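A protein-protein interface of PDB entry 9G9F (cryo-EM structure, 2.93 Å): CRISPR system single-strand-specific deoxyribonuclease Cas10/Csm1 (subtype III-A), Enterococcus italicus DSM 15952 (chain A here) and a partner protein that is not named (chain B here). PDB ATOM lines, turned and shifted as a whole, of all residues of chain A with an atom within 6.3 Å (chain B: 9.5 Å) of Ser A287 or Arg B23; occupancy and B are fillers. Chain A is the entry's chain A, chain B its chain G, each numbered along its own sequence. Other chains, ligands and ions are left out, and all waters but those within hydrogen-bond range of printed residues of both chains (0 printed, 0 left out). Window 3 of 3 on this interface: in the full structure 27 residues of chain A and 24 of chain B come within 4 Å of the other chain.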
ATOM      1  N   TYR A 284      20.683  13.768  -9.478  1.00  0.00           N
ATOM      2  CA  TYR A 284      19.338  14.064  -9.961  1.00  0.00           C
ATOM      3  C   TYR A 284      19.304  14.271 -11.472  1.00  0.00           C
ATOM      4  O   TYR A 284      18.579  15.124 -11.986  1.00  0.00           O
ATOM      5  CB  TYR A 284      18.766  15.273  -9.231  1.00  0.00           C
ATOM      6  CG  TYR A 284      18.402  14.960  -7.801  1.00  0.00           C
ATOM      7  CD1 TYR A 284      19.336  15.089  -6.785  1.00  0.00           C
ATOM      8  CD2 TYR A 284      17.136  14.507  -7.472  1.00  0.00           C
ATOM      9  CE1 TYR A 284      19.009  14.795  -5.480  1.00  0.00           C
ATOM     10  CE2 TYR A 284      16.804  14.211  -6.172  1.00  0.00           C
ATOM     11  CZ  TYR A 284      17.742  14.355  -5.181  1.00  0.00           C
ATOM     12  OH  TYR A 284      17.406  14.059  -3.885  1.00  0.00           O
ATOM     13  N   ASN A 285      20.098  13.489 -12.191  1.00  0.00           N
ATOM     14  CA  ASN A 285      19.924  13.305 -13.622  1.00  0.00           C
ATOM     15  C   ASN A 285      18.938  12.192 -13.929  1.00  0.00           C
ATOM     16  O   ASN A 285      18.984  11.619 -15.019  1.00  0.00           O
ATOM     17  CB  ASN A 285      21.269  13.004 -14.283  1.00  0.00           C
ATOM     18  CG  ASN A 285      21.719  14.108 -15.204  1.00  0.00           C
ATOM     19  OD1 ASN A 285      21.145  15.194 -15.206  1.00  0.00           O
ATOM     20  ND2 ASN A 285      22.757  13.845 -15.987  1.00  0.00           N
ATOM     21  N   ILE A 286      18.059  11.874 -12.980  1.00  0.00           N
ATOM     22  CA  ILE A 286      17.190  10.713 -13.094  1.00  0.00           C
ATOM     23  C   ILE A 286      15.920  11.086 -13.848  1.00  0.00           C
ATOM     24  O   ILE A 286      15.323  12.142 -13.606  1.00  0.00           O
ATOM     25  CB  ILE A 286      16.889  10.175 -11.687  1.00  0.00           C
ATOM     26  CG1 ILE A 286      16.258  11.268 -10.822  1.00  0.00           C
ATOM     27  CG2 ILE A 286      18.181   9.777 -11.034  1.00  0.00           C
ATOM     28  CD1 ILE A 286      14.783  11.118 -10.636  1.00  0.00           C
ATOM     29  N   SER A 287      15.506  10.225 -14.785  1.00  0.00           N
ATOM     30  CA  SER A 287      14.315  10.505 -15.578  1.00  0.00           C
ATOM     31  C   SER A 287      13.028  10.225 -14.818  1.00  0.00           C
ATOM     32  O   SER A 287      11.953  10.624 -15.278  1.00  0.00           O
ATOM     33  CB  SER A 287      14.318   9.694 -16.877  1.00  0.00           C
ATOM     34  OG  SER A 287      14.041   8.331 -16.623  1.00  0.00           O
ATOM     35  N   GLY A 288      13.111   9.556 -13.673  1.00  0.00           N
ATOM     36  CA  GLY A 288      11.953   9.215 -12.883  1.00  0.00           C
ATOM     37  C   GLY A 288      11.447   7.808 -13.101  1.00  0.00           C
ATOM     38  O   GLY A 288      10.637   7.329 -12.298  1.00  0.00           O
ATOM     39  N   SER A 289      11.904   7.136 -14.160  1.00  0.00           N
ATOM     40  CA  SER A 289      11.442   5.780 -14.433  1.00  0.00           C
ATOM     41  C   SER A 289      11.870   4.818 -13.333  1.00  0.00           C
ATOM     42  O   SER A 289      11.090   3.957 -12.916  1.00  0.00           O
ATOM     43  CB  SER A 289      11.961   5.310 -15.790  1.00  0.00           C
ATOM     44  OG  SER A 289      11.475   4.016 -16.099  1.00  0.00           O
ATOM     45  N   LYS A 290      13.107   4.941 -12.864  1.00  0.00           N
ATOM     46  CA  LYS A 290      13.662   4.124 -11.789  1.00  0.00           C
ATOM     47  C   LYS A 290      14.401   5.013 -10.803  1.00  0.00           C
ATOM     48  O   LYS A 290      15.549   4.766 -10.430  1.00  0.00           O
ATOM     49  CB  LYS A 290      14.563   3.033 -12.353  1.00  0.00           C
ATOM     50  CG  LYS A 290      13.801   1.813 -12.837  1.00  0.00           C
ATOM     51  CD  LYS A 290      14.669   0.921 -13.698  1.00  0.00           C
ATOM     52  CE  LYS A 290      15.017   1.604 -15.008  1.00  0.00           C
ATOM     53  NZ  LYS A 290      13.804   1.915 -15.814  1.00  0.00           N
ATOM     54  N   ALA A 291      13.718   6.075 -10.373  1.00  0.00           N
ATOM     55  CA  ALA A 291      14.364   7.158  -9.639  1.00  0.00           C
ATOM     56  C   ALA A 291      14.985   6.680  -8.334  1.00  0.00           C
ATOM     57  O   ALA A 291      16.090   7.102  -7.979  1.00  0.00           O
ATOM     58  CB  ALA A 291      13.346   8.261  -9.366  1.00  0.00           C
ATOM     59  N   SER A 294      18.158   4.707  -8.985  1.00  0.00           N
ATOM     60  CA  SER A 294      19.147   5.601  -9.569  1.00  0.00           C
ATOM     61  C   SER A 294      19.775   6.487  -8.505  1.00  0.00           C
ATOM     62  O   SER A 294      20.999   6.594  -8.422  1.00  0.00           O
ATOM     63  CB  SER A 294      18.505   6.453 -10.660  1.00  0.00           C
ATOM     64  OG  SER A 294      17.974   5.667 -11.706  1.00  0.00           O
ATOM     65  N   LYS A 425      17.500   7.447 -21.492  1.00  0.00           N
ATOM     66  CA  LYS A 425      16.490   8.316 -20.897  1.00  0.00           C
ATOM     67  C   LYS A 425      17.053   9.085 -19.706  1.00  0.00           C
ATOM     68  O   LYS A 425      16.845  10.298 -19.585  1.00  0.00           O
ATOM     69  CB  LYS A 425      15.261   7.503 -20.491  1.00  0.00           C
ATOM     70  CG  LYS A 425      15.555   6.117 -19.956  1.00  0.00           C
ATOM     71  CD  LYS A 425      14.273   5.310 -19.851  1.00  0.00           C
ATOM     72  CE  LYS A 425      14.522   3.938 -19.266  1.00  0.00           C
ATOM     73  NZ  LYS A 425      14.983   4.019 -17.856  1.00  0.00           N
ATOM     74  N   GLU A 426      17.782   8.400 -18.823  1.00  0.00           N
ATOM     75  CA  GLU A 426      18.349   9.056 -17.648  1.00  0.00           C
ATOM     76  C   GLU A 426      19.598   9.851 -18.006  1.00  0.00           C
ATOM     77  O   GLU A 426      19.632  11.077 -17.865  1.00  0.00           O
ATOM     78  CB  GLU A 426      18.684   8.021 -16.574  1.00  0.00           C
ATOM     79  CG  GLU A 426      17.599   7.784 -15.541  1.00  0.00           C
ATOM     80  CD  GLU A 426      16.609   6.724 -15.962  1.00  0.00           C
ATOM     81  OE1 GLU A 426      16.869   6.036 -16.969  1.00  0.00           O
ATOM     82  OE2 GLU A 426      15.583   6.559 -15.269  1.00  0.00           O
ATOM     83  N   CYS A 427      20.631   9.157 -18.484  1.00  0.00           N
ATOM     84  CA  CYS A 427      21.916   9.794 -18.749  1.00  0.00           C
ATOM     85  C   CYS A 427      21.793  10.903 -19.788  1.00  0.00           C
ATOM     86  O   CYS A 427      22.535  11.890 -19.732  1.00  0.00           O
ATOM     87  CB  CYS A 427      22.923   8.734 -19.205  1.00  0.00           C
ATOM     88  SG  CYS A 427      23.691   7.732 -17.892  1.00  0.00           S
ATOM     89  N   LEU A 428      20.861  10.764 -20.733  1.00  0.00           N
ATOM     90  CA  LEU A 428      20.624  11.747 -21.793  1.00  0.00           C
ATOM     91  C   LEU A 428      21.893  12.021 -22.595  1.00  0.00           C
ATOM     92  O   LEU A 428      22.350  13.159 -22.722  1.00  0.00           O
ATOM     93  CB  LEU A 428      20.045  13.043 -21.227  1.00  0.00           C
ATOM     94  CG  LEU A 428      18.520  13.132 -21.188  1.00  0.00           C
ATOM     95  CD1 LEU A 428      18.079  14.567 -20.983  1.00  0.00           C
ATOM     96  CD2 LEU A 428      17.918  12.560 -22.457  1.00  0.00           C
ATOM     97  N   SER A 649      10.625  11.657  -8.519  1.00  0.00           N
ATOM     98  CA  SER A 649      11.284  12.912  -8.867  1.00  0.00           C
ATOM     99  C   SER A 649      10.537  14.106  -8.286  1.00  0.00           C
ATOM    100  O   SER A 649      11.156  15.037  -7.752  1.00  0.00           O
ATOM    101  CB  SER A 649      11.398  13.039 -10.384  1.00  0.00           C
ATOM    102  OG  SER A 649      10.124  12.955 -10.994  1.00  0.00           O
ATOM    103  N   HIS B  18       8.106  28.043 -21.200  1.00  0.00           N
ATOM    104  CA  HIS B  18       8.750  26.804 -20.780  1.00  0.00           C
ATOM    105  C   HIS B  18      10.240  27.013 -20.542  1.00  0.00           C
ATOM    106  O   HIS B  18      10.727  26.850 -19.417  1.00  0.00           O
ATOM    107  CB  HIS B  18       8.528  25.704 -21.813  1.00  0.00           C
ATOM    108  CG  HIS B  18       9.129  24.395 -21.417  1.00  0.00           C
ATOM    109  ND1 HIS B  18      10.173  23.816 -22.101  1.00  0.00           N
ATOM    110  CD2 HIS B  18       8.842  23.559 -20.394  1.00  0.00           C
ATOM    111  CE1 HIS B  18      10.498  22.676 -21.520  1.00  0.00           C
ATOM    112  NE2 HIS B  18       9.704  22.496 -20.483  1.00  0.00           N
ATOM    113  N   PHE B  19      10.975  27.391 -21.585  1.00  0.00           N
ATOM    114  CA  PHE B  19      12.413  27.634 -21.501  1.00  0.00           C
ATOM    115  C   PHE B  19      13.135  26.464 -20.838  1.00  0.00           C
ATOM    116  O   PHE B  19      13.804  26.607 -19.815  1.00  0.00           O
ATOM    117  CB  PHE B  19      12.707  28.933 -20.755  1.00  0.00           C
ATOM    118  CG  PHE B  19      12.414  30.168 -21.537  1.00  0.00           C
ATOM    119  CD1 PHE B  19      12.144  30.107 -22.884  1.00  0.00           C
ATOM    120  CD2 PHE B  19      12.419  31.400 -20.919  1.00  0.00           C
ATOM    121  CE1 PHE B  19      11.888  31.254 -23.597  1.00  0.00           C
ATOM    122  CE2 PHE B  19      12.158  32.545 -21.627  1.00  0.00           C
ATOM    123  CZ  PHE B  19      11.892  32.472 -22.965  1.00  0.00           C
ATOM    124  N   GLY B  20      12.982  25.288 -21.428  1.00  0.00           N
ATOM    125  CA  GLY B  20      13.698  24.135 -20.935  1.00  0.00           C
ATOM    126  C   GLY B  20      15.185  24.248 -21.195  1.00  0.00           C
ATOM    127  O   GLY B  20      15.637  24.924 -22.118  1.00  0.00           O
ATOM    128  N   MET B  21      15.962  23.578 -20.353  1.00  0.00           N
ATOM    129  CA  MET B  21      17.412  23.544 -20.506  1.00  0.00           C
ATOM    130  C   MET B  21      17.939  22.153 -20.798  1.00  0.00           C
ATOM    131  O   MET B  21      18.871  22.004 -21.594  1.00  0.00           O
ATOM    132  CB  MET B  21      18.108  24.092 -19.250  1.00  0.00           C
ATOM    133  CG  MET B  21      17.595  23.520 -17.935  1.00  0.00           C
ATOM    134  SD  MET B  21      17.495  24.754 -16.624  1.00  0.00           S
ATOM    135  CE  MET B  21      16.600  23.851 -15.369  1.00  0.00           C
ATOM    136  N   LYS B  22      17.374  21.129 -20.163  1.00  0.00           N
ATOM    137  CA  LYS B  22      17.729  19.747 -20.461  1.00  0.00           C
ATOM    138  C   LYS B  22      16.541  18.808 -20.600  1.00  0.00           C
ATOM    139  O   LYS B  22      16.705  17.731 -21.180  1.00  0.00           O
ATOM    140  CB  LYS B  22      18.681  19.206 -19.390  1.00  0.00           C
ATOM    141  CG  LYS B  22      19.512  18.024 -19.829  1.00  0.00           C
ATOM    142  CD  LYS B  22      20.395  17.543 -18.698  1.00  0.00           C
ATOM    143  CE  LYS B  22      19.589  17.122 -17.489  1.00  0.00           C
ATOM    144  NZ  LYS B  22      18.684  15.982 -17.777  1.00  0.00           N
ATOM    145  N   ARG B  23      15.357  19.158 -20.104  1.00  0.00           N
ATOM    146  CA  ARG B  23      14.193  18.281 -20.161  1.00  0.00           C
ATOM    147  C   ARG B  23      12.941  19.118 -20.386  1.00  0.00           C
ATOM    148  O   ARG B  23      13.006  20.277 -20.800  1.00  0.00           O
ATOM    149  CB  ARG B  23      14.055  17.448 -18.885  1.00  0.00           C
ATOM    150  CG  ARG B  23      15.276  16.686 -18.477  1.00  0.00           C
ATOM    151  CD  ARG B  23      14.997  15.985 -17.179  1.00  0.00           C
ATOM    152  NE  ARG B  23      16.013  14.986 -16.886  1.00  0.00           N
ATOM    153  CZ  ARG B  23      15.762  13.878 -16.207  1.00  0.00           C
ATOM    154  NH1 ARG B  23      14.556  13.630 -15.724  1.00  0.00           N
ATOM    155  NH2 ARG B  23      16.731  12.987 -16.032  1.00  0.00           N
ATOM    156  N   LEU B  24      11.789  18.507 -20.121  1.00  0.00           N
ATOM    157  CA  LEU B  24      10.508  19.201 -20.163  1.00  0.00           C
ATOM    158  C   LEU B  24       9.994  19.555 -18.777  1.00  0.00           C
ATOM    159  O   LEU B  24       9.243  20.524 -18.630  1.00  0.00           O
ATOM    160  CB  LEU B  24       9.463  18.339 -20.877  1.00  0.00           C
ATOM    161  CG  LEU B  24       8.162  18.971 -21.379  1.00  0.00           C
ATOM    162  CD1 LEU B  24       8.388  19.835 -22.601  1.00  0.00           C
ATOM    163  CD2 LEU B  24       7.133  17.894 -21.668  1.00  0.00           C
ATOM    164  N   SER B  25      10.385  18.798 -17.755  1.00  0.00           N
ATOM    165  CA  SER B  25       9.872  19.042 -16.417  1.00  0.00           C
ATOM    166  C   SER B  25      10.536  20.227 -15.734  1.00  0.00           C
ATOM    167  O   SER B  25      10.081  20.627 -14.661  1.00  0.00           O
ATOM    168  CB  SER B  25      10.045  17.794 -15.555  1.00  0.00           C
ATOM    169  OG  SER B  25       9.498  16.657 -16.195  1.00  0.00           O
ATOM    170  N   ASP B  26      11.594  20.786 -16.313  1.00  0.00           N
ATOM    171  CA  ASP B  26      12.281  21.934 -15.741  1.00  0.00           C
ATOM    172  C   ASP B  26      11.905  23.208 -16.486  1.00  0.00           C
ATOM    173  O   ASP B  26      11.309  23.176 -17.563  1.00  0.00           O
ATOM    174  CB  ASP B  26      13.798  21.725 -15.763  1.00  0.00           C
ATOM    175  CG  ASP B  26      14.341  21.457 -17.154  1.00  0.00           C
ATOM    176  OD1 ASP B  26      13.611  21.644 -18.146  1.00  0.00           O
ATOM    177  OD2 ASP B  26      15.518  21.056 -17.253  1.00  0.00           O
ATOM    178  N   SER B  27      12.261  24.347 -15.894  1.00  0.00           N
ATOM    179  CA  SER B  27      11.959  25.639 -16.506  1.00  0.00           C
ATOM    180  C   SER B  27      13.043  26.630 -16.100  1.00  0.00           C
ATOM    181  O   SER B  27      12.965  27.231 -15.025  1.00  0.00           O
ATOM    182  CB  SER B  27      10.584  26.135 -16.091  1.00  0.00           C
ATOM    183  OG  SER B  27      10.278  27.368 -16.716  1.00  0.00           O
ATOM    184  N   ASN B  28      14.039  26.798 -16.961  1.00  0.00           N
ATOM    185  CA  ASN B  28      14.960  27.909 -16.800  1.00  0.00           C
ATOM    186  C   ASN B  28      14.210  29.216 -17.018  1.00  0.00           C
ATOM    187  O   ASN B  28      13.175  29.258 -17.686  1.00  0.00           O
ATOM    188  CB  ASN B  28      16.120  27.778 -17.785  1.00  0.00           C
ATOM    189  CG  ASN B  28      17.281  28.675 -17.441  1.00  0.00           C
ATOM    190  OD1 ASN B  28      17.611  29.593 -18.186  1.00  0.00           O
ATOM    191  ND2 ASN B  28      17.910  28.419 -16.301  1.00  0.00           N
ATOM    192  N   LEU B 131       5.338  24.160 -11.922  1.00  0.00           N
ATOM    193  CA  LEU B 131       5.286  22.944 -12.721  1.00  0.00           C
ATOM    194  C   LEU B 131       3.828  22.581 -12.947  1.00  0.00           C
ATOM    195  O   LEU B 131       3.107  22.290 -11.989  1.00  0.00           O
ATOM    196  CB  LEU B 131       6.025  21.802 -12.022  1.00  0.00           C
ATOM    197  CG  LEU B 131       6.097  20.455 -12.734  1.00  0.00           C
ATOM    198  CD1 LEU B 131       7.535  20.002 -12.856  1.00  0.00           C
ATOM    199  CD2 LEU B 131       5.275  19.429 -11.986  1.00  0.00           C
ATOM    200  N   SER B 150       4.531  16.351 -17.472  1.00  0.00           N
ATOM    201  CA  SER B 150       4.581  17.622 -16.769  1.00  0.00           C
ATOM    202  C   SER B 150       5.446  18.599 -17.543  1.00  0.00           C
ATOM    203  O   SER B 150       6.480  18.220 -18.098  1.00  0.00           O
ATOM    204  CB  SER B 150       5.122  17.456 -15.348  1.00  0.00           C
ATOM    205  OG  SER B 150       6.336  16.731 -15.351  1.00  0.00           O
ATOM    206  N   VAL B 151       5.018  19.854 -17.577  1.00  0.00           N
ATOM    207  CA  VAL B 151       5.733  20.923 -18.255  1.00  0.00           C
ATOM    208  C   VAL B 151       6.062  21.987 -17.221  1.00  0.00           C
ATOM    209  O   VAL B 151       5.175  22.449 -16.495  1.00  0.00           O
ATOM    210  CB  VAL B 151       4.905  21.511 -19.411  1.00  0.00           C
ATOM    211  CG1 VAL B 151       5.695  22.556 -20.153  1.00  0.00           C
ATOM    212  CG2 VAL B 151       4.488  20.415 -20.355  1.00  0.00           C
ATOM    213  N   GLY B 152       7.331  22.362 -17.143  1.00  0.00           N
ATOM    214  CA  GLY B 152       7.731  23.392 -16.212  1.00  0.00           C
ATOM    215  C   GLY B 152       7.637  24.760 -16.845  1.00  0.00           C
ATOM    216  O   GLY B 152       8.225  24.993 -17.902  1.00  0.00           O
ATOM    217  N   ASN B 153       6.902  25.675 -16.220  1.00  0.00           N
ATOM    218  CA  ASN B 153       6.737  27.017 -16.746  1.00  0.00           C
ATOM    219  C   ASN B 153       7.268  28.036 -15.747  1.00  0.00           C
ATOM    220  O   ASN B 153       7.500  27.729 -14.577  1.00  0.00           O
ATOM    221  CB  ASN B 153       5.270  27.312 -17.081  1.00  0.00           C
ATOM    222  CG  ASN B 153       4.314  26.755 -16.054  1.00  0.00           C
ATOM    223  OD1 ASN B 153       3.858  25.621 -16.167  1.00  0.00           O
ATOM    224  ND2 ASN B 153       3.994  27.557 -15.050  1.00  0.00           N
ATOM    225  N   GLY B 189      10.639  29.737 -26.705  1.00  0.00           N
ATOM    226  CA  GLY B 189      10.746  28.639 -25.772  1.00  0.00           C
ATOM    227  C   GLY B 189       9.989  27.412 -26.238  1.00  0.00           C
ATOM    228  O   GLY B 189       9.326  27.399 -27.275  1.00  0.00           O
ATOM    229  N   GLY B 190      10.101  26.352 -25.450  1.00  0.00           N
ATOM    230  CA  GLY B 190       9.407  25.126 -25.771  1.00  0.00           C
ATOM    231  C   GLY B 190       7.921  25.226 -25.508  1.00  0.00           C
ATOM    232  O   GLY B 190       7.440  26.128 -24.827  1.00  0.00           O
ATOM    233  N   LYS B 191       7.183  24.273 -26.073  1.00  0.00           N
ATOM    234  CA  LYS B 191       5.725  24.223 -25.952  1.00  0.00           C
ATOM    235  C   LYS B 191       5.079  25.525 -26.407  1.00  0.00           C
ATOM    236  O   LYS B 191       4.051  25.941 -25.877  1.00  0.00           O
ATOM    237  CB  LYS B 191       5.296  23.881 -24.525  1.00  0.00           C
ATOM    238  CG  LYS B 191       4.624  22.533 -24.384  1.00  0.00           C
ATOM    239  CD  LYS B 191       5.448  21.440 -25.028  1.00  0.00           C
ATOM    240  CE  LYS B 191       4.912  20.065 -24.682  1.00  0.00           C
ATOM    241  NZ  LYS B 191       3.522  19.865 -25.159  1.00  0.00           N
ATOM    242  N   ARG B 247      25.421  22.569 -24.698  1.00  0.00           N
ATOM    243  CA  ARG B 247      24.303  22.926 -25.563  1.00  0.00           C
ATOM    244  C   ARG B 247      24.024  21.752 -26.495  1.00  0.00           C
ATOM    245  O   ARG B 247      24.889  21.352 -27.284  1.00  0.00           O
ATOM    246  CB  ARG B 247      24.611  24.195 -26.349  1.00  0.00           C
ATOM    247  CG  ARG B 247      25.321  25.261 -25.544  1.00  0.00           C
ATOM    248  CD  ARG B 247      24.453  25.749 -24.397  1.00  0.00           C
ATOM    249  NE  ARG B 247      23.269  26.466 -24.855  1.00  0.00           N
ATOM    250  CZ  ARG B 247      22.023  26.137 -24.541  1.00  0.00           C
ATOM    251  NH1 ARG B 247      21.757  25.104 -23.759  1.00  0.00           N
ATOM    252  NH2 ARG B 247      21.020  26.862 -25.023  1.00  0.00           N
ATOM    253  N   THR B 248      22.819  21.196 -26.393  1.00  0.00           N
ATOM    254  CA  THR B 248      22.396  20.056 -27.192  1.00  0.00           C
ATOM    255  C   THR B 248      20.942  20.279 -27.594  1.00  0.00           C
ATOM    256  O   THR B 248      20.391  21.370 -27.421  1.00  0.00           O
ATOM    257  CB  THR B 248      22.575  18.748 -26.410  1.00  0.00           C
ATOM    258  OG1 THR B 248      22.163  18.947 -25.053  1.00  0.00           O
ATOM    259  CG2 THR B 248      24.027  18.301 -26.436  1.00  0.00           C
ATOM    260  N   GLY B 249      20.316  19.247 -28.131  1.00  0.00           N
ATOM    261  CA  GLY B 249      18.893  19.270 -28.419  1.00  0.00           C
ATOM    262  C   GLY B 249      18.572  18.623 -29.752  1.00  0.00           C
ATOM    263  O   GLY B 249      19.446  18.350 -30.573  1.00  0.00           O
ATOM    264  N   PHE B 250      17.283  18.371 -29.964  1.00  0.00           N
ATOM    265  CA  PHE B 250      16.792  17.837 -31.223  1.00  0.00           C
ATOM    266  C   PHE B 250      16.585  18.959 -32.232  1.00  0.00           C
ATOM    267  O   PHE B 250      16.473  20.135 -31.878  1.00  0.00           O
ATOM    268  CB  PHE B 250      15.476  17.094 -31.021  1.00  0.00           C
ATOM    269  CG  PHE B 250      15.617  15.766 -30.342  1.00  0.00           C
ATOM    270  CD1 PHE B 250      15.925  15.688 -28.999  1.00  0.00           C
ATOM    271  CD2 PHE B 250      15.415  14.593 -31.044  1.00  0.00           C
ATOM    272  CE1 PHE B 250      16.042  14.467 -28.375  1.00  0.00           C
ATOM    273  CE2 PHE B 250      15.530  13.371 -30.425  1.00  0.00           C
ATOM    274  CZ  PHE B 250      15.844  13.307 -29.090  1.00  0.00           C
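Of the 14 printed residues of chain A, 5 touch a printed residue of chain B.
Among the printed residues, no Asp or Glu carboxylate lies within 4 Å of a Lys or Arg side-chain nitrogen of the other chain.
Ser A287 touches just one residue of chain B: Arg B23 (3.1 Å).
Ile A286 touches just one residue of chain B: Arg B23.
No residue of chain B comes within 4 Å of Gly A288.
Of the printed residues of chain A, Lys B22 touches Asn A285 (3.4 Å) and Leu A428 (3.5 Å).
Of the printed residues of chain B, Asn A285 touches Lys B22 and Arg B23.
Of the printed residues of chain B, Leu A428 touches Lys B22.
Gly B190 touches none of the printed residues of chain A.
OG of Ser A287 lies within hydrogen-bond range of OE2 of Glu A426.
N of Arg B23 sits at hydrogen-bond distance from OD2 of Asp B26.
The backbone NH (N) of Ser A289 sits close to the side-chain hydroxyl (OG) of Ser A287 (3.5 Å).
The backbone NH of Lys B22 is in hydrogen-bond range of the side-chain carboxylate of Asp B26 (3.5 Å).
NZ of Lys A425 is in salt-bridge range of OE1 of Glu A426.
Lys B22 touches Asn A285 (CE to OD1, 3.4 Å).
NH2 of Arg B23 touches O of Glu A426, 3.9 Å away.
Lys B22 touches Leu A428 (O to CD1, 3.5 Å).
O of Ile A286 lies within hydrogen-bond range of NH1 of Arg B23, at 2.7 Å.
The backbone carbonyl oxygen (O) of Asn A285 sits at hydrogen-bond distance from the guanidinium group (NH2) of Arg B23, 2.8 Å away.
The backbone NH of Ser A287 lies close to the guanidinium group of Arg B23, 3.3 Å away.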
